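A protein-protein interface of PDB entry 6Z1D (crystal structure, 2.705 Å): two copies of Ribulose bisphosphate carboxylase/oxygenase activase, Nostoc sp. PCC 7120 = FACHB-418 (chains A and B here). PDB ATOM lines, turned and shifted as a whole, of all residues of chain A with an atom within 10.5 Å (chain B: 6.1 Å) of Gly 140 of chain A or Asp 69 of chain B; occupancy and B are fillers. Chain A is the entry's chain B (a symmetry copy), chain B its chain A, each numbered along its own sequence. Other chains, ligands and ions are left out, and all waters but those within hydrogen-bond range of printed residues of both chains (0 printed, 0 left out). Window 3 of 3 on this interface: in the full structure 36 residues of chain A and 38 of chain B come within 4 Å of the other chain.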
ATOM      1  N   ASP A  72      17.232   0.877 -23.010  1.00  0.00           N
ATOM      2  CA  ASP A  72      17.590  -0.007 -21.910  1.00  0.00           C
ATOM      3  C   ASP A  72      17.938  -1.396 -22.428  1.00  0.00           C
ATOM      4  O   ASP A  72      17.047  -2.177 -22.762  1.00  0.00           O
ATOM      5  CB  ASP A  72      16.427  -0.106 -20.923  1.00  0.00           C
ATOM      6  CG  ASP A  72      16.851  -0.624 -19.570  1.00  0.00           C
ATOM      7  OD1 ASP A  72      17.803  -1.433 -19.503  1.00  0.00           O
ATOM      8  OD2 ASP A  72      16.223  -0.213 -18.569  1.00  0.00           O
ATOM      9  N   ALA A  74      19.573  -3.824 -20.674  1.00  0.00           N
ATOM     10  CA  ALA A  74      19.323  -4.835 -19.656  1.00  0.00           C
ATOM     11  C   ALA A  74      17.903  -5.357 -19.827  1.00  0.00           C
ATOM     12  O   ALA A  74      17.663  -6.563 -19.874  1.00  0.00           O
ATOM     13  CB  ALA A  74      19.510  -4.261 -18.276  1.00  0.00           C
ATOM     14  N   ARG A  75      16.964  -4.428 -19.935  1.00  0.00           N
ATOM     15  CA  ARG A  75      15.564  -4.767 -20.121  1.00  0.00           C
ATOM     16  C   ARG A  75      15.385  -5.662 -21.352  1.00  0.00           C
ATOM     17  O   ARG A  75      14.768  -6.729 -21.273  1.00  0.00           O
ATOM     18  CB  ARG A  75      14.749  -3.482 -20.259  1.00  0.00           C
ATOM     19  CG  ARG A  75      13.261  -3.684 -20.415  1.00  0.00           C
ATOM     20  CD  ARG A  75      12.552  -2.342 -20.417  1.00  0.00           C
ATOM     21  NE  ARG A  75      11.106  -2.462 -20.596  1.00  0.00           N
ATOM     22  CZ  ARG A  75      10.504  -2.558 -21.780  1.00  0.00           C
ATOM     23  NH1 ARG A  75      11.215  -2.560 -22.904  1.00  0.00           N
ATOM     24  NH2 ARG A  75       9.183  -2.658 -21.845  1.00  0.00           N
ATOM     25  N   ARG A  78      16.555  -9.161 -20.919  1.00  0.00           N
ATOM     26  CA  ARG A  78      15.719  -9.880 -19.975  1.00  0.00           C
ATOM     27  C   ARG A  78      14.361 -10.213 -20.574  1.00  0.00           C
ATOM     28  O   ARG A  78      13.805 -11.274 -20.286  1.00  0.00           O
ATOM     29  CB  ARG A  78      15.557  -9.075 -18.693  1.00  0.00           C
ATOM     30  CG  ARG A  78      16.800  -9.101 -17.845  1.00  0.00           C
ATOM     31  CD  ARG A  78      16.696  -8.168 -16.668  1.00  0.00           C
ATOM     32  NE  ARG A  78      17.773  -8.372 -15.702  1.00  0.00           N
ATOM     33  CZ  ARG A  78      17.846  -9.398 -14.860  1.00  0.00           C
ATOM     34  NH1 ARG A  78      16.917 -10.339 -14.866  1.00  0.00           N
ATOM     35  NH2 ARG A  78      18.853  -9.488 -14.009  1.00  0.00           N
ATOM     36  N   ARG A  82      13.117 -14.168 -21.096  1.00  0.00           N
ATOM     37  CA  ARG A  82      11.836 -14.662 -20.593  1.00  0.00           C
ATOM     38  C   ARG A  82      10.930 -15.134 -21.721  1.00  0.00           C
ATOM     39  O   ARG A  82      10.161 -16.082 -21.563  1.00  0.00           O
ATOM     40  CB  ARG A  82      11.126 -13.576 -19.789  1.00  0.00           C
ATOM     41  CG  ARG A  82      11.898 -13.152 -18.562  1.00  0.00           C
ATOM     42  CD  ARG A  82      11.122 -12.166 -17.712  1.00  0.00           C
ATOM     43  NE  ARG A  82      10.401 -12.877 -16.664  1.00  0.00           N
ATOM     44  CZ  ARG A  82       9.118 -13.207 -16.720  1.00  0.00           C
ATOM     45  NH1 ARG A  82       8.374 -12.870 -17.769  1.00  0.00           N
ATOM     46  NH2 ARG A  82       8.572 -13.867 -15.708  1.00  0.00           N
ATOM     47  N   VAL A 136      14.780 -15.143 -13.666  1.00  0.00           N
ATOM     48  CA  VAL A 136      15.101 -13.967 -14.463  1.00  0.00           C
ATOM     49  C   VAL A 136      13.896 -13.050 -14.553  1.00  0.00           C
ATOM     50  O   VAL A 136      12.981 -13.293 -15.337  1.00  0.00           O
ATOM     51  CB  VAL A 136      15.541 -14.356 -15.878  1.00  0.00           C
ATOM     52  CG1 VAL A 136      15.860 -13.118 -16.706  1.00  0.00           C
ATOM     53  CG2 VAL A 136      16.751 -15.270 -15.808  1.00  0.00           C
ATOM     54  N   GLN A 137      13.928 -11.981 -13.762  1.00  0.00           N
ATOM     55  CA  GLN A 137      12.817 -11.046 -13.647  1.00  0.00           C
ATOM     56  C   GLN A 137      13.094  -9.801 -14.461  1.00  0.00           C
ATOM     57  O   GLN A 137      14.244  -9.373 -14.559  1.00  0.00           O
ATOM     58  CB  GLN A 137      12.657 -10.632 -12.185  1.00  0.00           C
ATOM     59  CG  GLN A 137      12.448 -11.797 -11.241  1.00  0.00           C
ATOM     60  CD  GLN A 137      11.123 -12.474 -11.482  1.00  0.00           C
ATOM     61  OE1 GLN A 137      10.214 -11.889 -12.081  1.00  0.00           O
ATOM     62  NE2 GLN A 137      11.003 -13.717 -11.028  1.00  0.00           N
ATOM     63  N   LEU A 138      12.058  -9.203 -15.038  1.00  0.00           N
ATOM     64  CA  LEU A 138      12.221  -7.893 -15.648  1.00  0.00           C
ATOM     65  C   LEU A 138      12.494  -6.875 -14.534  1.00  0.00           C
ATOM     66  O   LEU A 138      11.975  -7.007 -13.431  1.00  0.00           O
ATOM     67  CB  LEU A 138      10.977  -7.492 -16.428  1.00  0.00           C
ATOM     68  CG  LEU A 138      10.505  -8.417 -17.542  1.00  0.00           C
ATOM     69  CD1 LEU A 138       9.435  -7.683 -18.298  1.00  0.00           C
ATOM     70  CD2 LEU A 138      11.650  -8.818 -18.460  1.00  0.00           C
ATOM     71  N   PRO A 139      13.290  -5.842 -14.816  1.00  0.00           N
ATOM     72  CA  PRO A 139      13.562  -4.858 -13.761  1.00  0.00           C
ATOM     73  C   PRO A 139      12.281  -4.205 -13.221  1.00  0.00           C
ATOM     74  O   PRO A 139      11.456  -3.724 -14.004  1.00  0.00           O
ATOM     75  CB  PRO A 139      14.458  -3.847 -14.465  1.00  0.00           C
ATOM     76  CG  PRO A 139      14.062  -3.955 -15.936  1.00  0.00           C
ATOM     77  CD  PRO A 139      13.772  -5.409 -16.136  1.00  0.00           C
ATOM     78  N   GLY A 140      12.112  -4.233 -11.899  1.00  0.00           N
ATOM     79  CA  GLY A 140      10.946  -3.667 -11.241  1.00  0.00           C
ATOM     80  C   GLY A 140       9.826  -4.667 -11.040  1.00  0.00           C
ATOM     81  O   GLY A 140       8.841  -4.394 -10.344  1.00  0.00           O
ATOM     82  N   SER A 141       9.988  -5.832 -11.647  1.00  0.00           N
ATOM     83  CA  SER A 141       8.981  -6.879 -11.593  1.00  0.00           C
ATOM     84  C   SER A 141       9.439  -8.012 -10.691  1.00  0.00           C
ATOM     85  O   SER A 141      10.639  -8.231 -10.513  1.00  0.00           O
ATOM     86  CB  SER A 141       8.729  -7.421 -12.998  1.00  0.00           C
ATOM     87  OG  SER A 141       8.474  -6.366 -13.909  1.00  0.00           O
ATOM     88  N   TYR A 142       8.478  -8.722 -10.113  1.00  0.00           N
ATOM     89  CA  TYR A 142       8.782  -9.953  -9.407  1.00  0.00           C
ATOM     90  C   TYR A 142       7.701 -10.991  -9.601  1.00  0.00           C
ATOM     91  O   TYR A 142       6.507 -10.724  -9.467  1.00  0.00           O
ATOM     92  CB  TYR A 142       9.003  -9.741  -7.908  1.00  0.00           C
ATOM     93  CG  TYR A 142       9.535 -11.001  -7.263  1.00  0.00           C
ATOM     94  CD1 TYR A 142      10.850 -11.402  -7.477  1.00  0.00           C
ATOM     95  CD2 TYR A 142       8.719 -11.813  -6.482  1.00  0.00           C
ATOM     96  CE1 TYR A 142      11.343 -12.558  -6.917  1.00  0.00           C
ATOM     97  CE2 TYR A 142       9.203 -12.974  -5.913  1.00  0.00           C
ATOM     98  CZ  TYR A 142      10.515 -13.342  -6.136  1.00  0.00           C
ATOM     99  OH  TYR A 142      11.018 -14.498  -5.580  1.00  0.00           O
ATOM    100  N   ASP A 143       8.164 -12.198  -9.885  1.00  0.00           N
ATOM    101  CA  ASP A 143       7.315 -13.318 -10.200  1.00  0.00           C
ATOM    102  C   ASP A 143       7.862 -14.525  -9.456  1.00  0.00           C
ATOM    103  O   ASP A 143       8.989 -14.942  -9.695  1.00  0.00           O
ATOM    104  CB  ASP A 143       7.365 -13.554 -11.705  1.00  0.00           C
ATOM    105  CG  ASP A 143       6.293 -14.486 -12.183  1.00  0.00           C
ATOM    106  OD1 ASP A 143       5.722 -15.224 -11.351  1.00  0.00           O
ATOM    107  OD2 ASP A 143       6.022 -14.478 -13.401  1.00  0.00           O
ATOM    108  N   SER A 144       7.061 -15.070  -8.547  1.00  0.00           N
ATOM    109  CA  SER A 144       7.434 -16.254  -7.779  1.00  0.00           C
ATOM    110  C   SER A 144       7.750 -17.446  -8.688  1.00  0.00           C
ATOM    111  O   SER A 144       8.430 -18.385  -8.281  1.00  0.00           O
ATOM    112  CB  SER A 144       6.306 -16.637  -6.826  1.00  0.00           C
ATOM    113  OG  SER A 144       5.078 -16.726  -7.530  1.00  0.00           O
ATOM    114  N   GLU B  64      13.195  -9.438  -4.839  1.00  0.00           N
ATOM    115  CA  GLU B  64      11.877  -9.203  -4.266  1.00  0.00           C
ATOM    116  C   GLU B  64      11.847  -7.786  -3.712  1.00  0.00           C
ATOM    117  O   GLU B  64      10.949  -6.998  -4.021  1.00  0.00           O
ATOM    118  CB  GLU B  64      11.620 -10.212  -3.145  1.00  0.00           C
ATOM    119  CG  GLU B  64      10.200 -10.753  -3.084  1.00  0.00           C
ATOM    120  CD  GLU B  64      10.088 -12.068  -2.322  1.00  0.00           C
ATOM    121  OE1 GLU B  64      11.128 -12.657  -1.939  1.00  0.00           O
ATOM    122  OE2 GLU B  64       8.938 -12.514  -2.108  1.00  0.00           O
ATOM    123  N   GLU B  66      13.765  -5.488  -4.493  1.00  0.00           N
ATOM    124  CA  GLU B  66      14.095  -4.541  -5.551  1.00  0.00           C
ATOM    125  C   GLU B  66      12.835  -4.094  -6.294  1.00  0.00           C
ATOM    126  O   GLU B  66      12.867  -3.152  -7.088  1.00  0.00           O
ATOM    127  CB  GLU B  66      15.088  -5.171  -6.535  1.00  0.00           C
ATOM    128  CG  GLU B  66      15.964  -4.164  -7.282  1.00  0.00           C
ATOM    129  CD  GLU B  66      16.685  -4.773  -8.478  1.00  0.00           C
ATOM    130  OE1 GLU B  66      16.075  -5.598  -9.192  1.00  0.00           O
ATOM    131  OE2 GLU B  66      17.866  -4.424  -8.705  1.00  0.00           O
ATOM    132  N   SER B  67      11.721  -4.765  -6.020  1.00  0.00           N
ATOM    133  CA  SER B  67      10.522  -4.602  -6.829  1.00  0.00           C
ATOM    134  C   SER B  67       9.379  -3.838  -6.141  1.00  0.00           C
ATOM    135  O   SER B  67       9.069  -4.095  -4.974  1.00  0.00           O
ATOM    136  CB  SER B  67      10.016  -5.978  -7.250  1.00  0.00           C
ATOM    137  OG  SER B  67       8.872  -5.856  -8.076  1.00  0.00           O
ATOM    138  N   PRO B  68       8.760  -2.884  -6.864  1.00  0.00           N
ATOM    139  CA  PRO B  68       7.451  -2.372  -6.461  1.00  0.00           C
ATOM    140  C   PRO B  68       6.431  -3.487  -6.236  1.00  0.00           C
ATOM    141  O   PRO B  68       5.545  -3.346  -5.388  1.00  0.00           O
ATOM    142  CB  PRO B  68       7.026  -1.552  -7.677  1.00  0.00           C
ATOM    143  CG  PRO B  68       8.287  -1.023  -8.234  1.00  0.00           C
ATOM    144  CD  PRO B  68       9.376  -2.025  -7.898  1.00  0.00           C
ATOM    145  N   ASP B  69       6.539  -4.558  -7.021  1.00  0.00           N
ATOM    146  CA  ASP B  69       5.537  -5.630  -7.007  1.00  0.00           C
ATOM    147  C   ASP B  69       5.610  -6.486  -5.748  1.00  0.00           C
ATOM    148  O   ASP B  69       4.799  -7.391  -5.552  1.00  0.00           O
ATOM    149  CB  ASP B  69       5.646  -6.509  -8.258  1.00  0.00           C
ATOM    150  CG  ASP B  69       5.269  -5.766  -9.539  1.00  0.00           C
ATOM    151  OD1 ASP B  69       4.878  -4.580  -9.455  1.00  0.00           O
ATOM    152  OD2 ASP B  69       5.340  -6.385 -10.629  1.00  0.00           O
ATOM    153  N   ALA B  70       6.590  -6.184  -4.906  1.00  0.00           N
ATOM    154  CA  ALA B  70       6.624  -6.681  -3.541  1.00  0.00           C
ATOM    155  C   ALA B  70       6.003  -5.621  -2.626  1.00  0.00           C
ATOM    156  O   ALA B  70       5.939  -5.788  -1.406  1.00  0.00           O
ATOM    157  CB  ALA B  70       8.058  -6.961  -3.141  1.00  0.00           C
ATOM    158  N   GLY B  71       5.542  -4.530  -3.235  1.00  0.00           N
ATOM    159  CA  GLY B  71       5.024  -3.393  -2.501  1.00  0.00           C
ATOM    160  C   GLY B  71       6.085  -2.732  -1.647  1.00  0.00           C
ATOM    161  O   GLY B  71       7.252  -2.655  -2.028  1.00  0.00           O
ATOM    162  N   TYR B 115      15.382   0.894 -11.088  1.00  0.00           N
ATOM    163  CA  TYR B 115      15.024   0.180  -9.862  1.00  0.00           C
ATOM    164  C   TYR B 115      16.234  -0.387  -9.148  1.00  0.00           C
ATOM    165  O   TYR B 115      17.060  -1.079  -9.745  1.00  0.00           O
ATOM    166  CB  TYR B 115      14.042  -0.963 -10.160  1.00  0.00           C
ATOM    167  CG  TYR B 115      13.056  -0.675 -11.282  1.00  0.00           C
ATOM    168  CD1 TYR B 115      11.756  -0.279 -11.015  1.00  0.00           C
ATOM    169  CD2 TYR B 115      13.422  -0.798 -12.599  1.00  0.00           C
ATOM    170  CE1 TYR B 115      10.853  -0.015 -12.035  1.00  0.00           C
ATOM    171  CE2 TYR B 115      12.525  -0.532 -13.624  1.00  0.00           C
ATOM    172  CZ  TYR B 115      11.243  -0.143 -13.340  1.00  0.00           C
ATOM    173  OH  TYR B 115      10.363   0.123 -14.382  1.00  0.00           O
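The backbone carbonyl oxygen of Gly 140 of chain A lies within hydrogen-bond range of the side-chain hydroxyl of Ser 67 of chain B (2.7 Å).
The side-chain hydroxyl of Ser 67 of chain B is in hydrogen-bond range of the backbone NH of Asp 69 of chain B.
Among the printed residues, pairs that only touch across the chains: Pro 139 of chain A with Tyr 115 of chain B, Gly 140 of chain A with Pro 68 of chain B, Gly 140 of chain A with Asp 69 of chain B, Gly 140 of chain A with Tyr 115 of chain B, Ser 141 of chain A with Ser 67 of chain B, Ser 141 of chain A with Asp 69 of chain B, Tyr 142 of chain A with Glu 64 of chain B, Tyr 142 of chain A with Ser 67 of chain B and Tyr 142 of chain A with Asp 69 of chain B.
Hydrophobic or aromatic side chains of chain A that line the printed part of chain B: Pro 139 and Tyr 142.
Among the printed residues, no Asp or Glu carboxylate lies within 4 Å of a Lys or Arg side-chain nitrogen of the other chain.
No position is printed for both chains.
Of the printed residues of chain B, Gly 140 of chain A touches Ser 67, Pro 68, Asp 69 and Tyr 115.
Of the printed residues of chain A, Asp 69 of chain B touches Gly 140, Ser 141 and Tyr 142.
Printed residues of chain A within 4 Å of Ser 67 of chain B: Gly 140, Ser 141 and Tyr 142.
Ala 70 of chain B touches none of the printed residues of chain A.
Gly 71 of chain B touches none of the printed residues of chain A.
Printed residues of chain A within 4 Å of Tyr 115 of chain B: Pro 139 (3.4 Å) and Gly 140 (3.5 Å).
Of the printed residues of chain B, Ser 141 of chain A touches Ser 67 and Asp 69.
Of the printed residues of chain A, Glu 64 of chain B touches Tyr 142.
Printed residues of chain B within 4 Å of Tyr 142 of chain A: Glu 64, Ser 67 and Asp 69.
Arg 82 of chain A touches none of the printed residues of chain B.
The nearest printed residue of chain B that does not touch Pro 139 of chain A is Glu 66 of chain B (5.3 Å).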
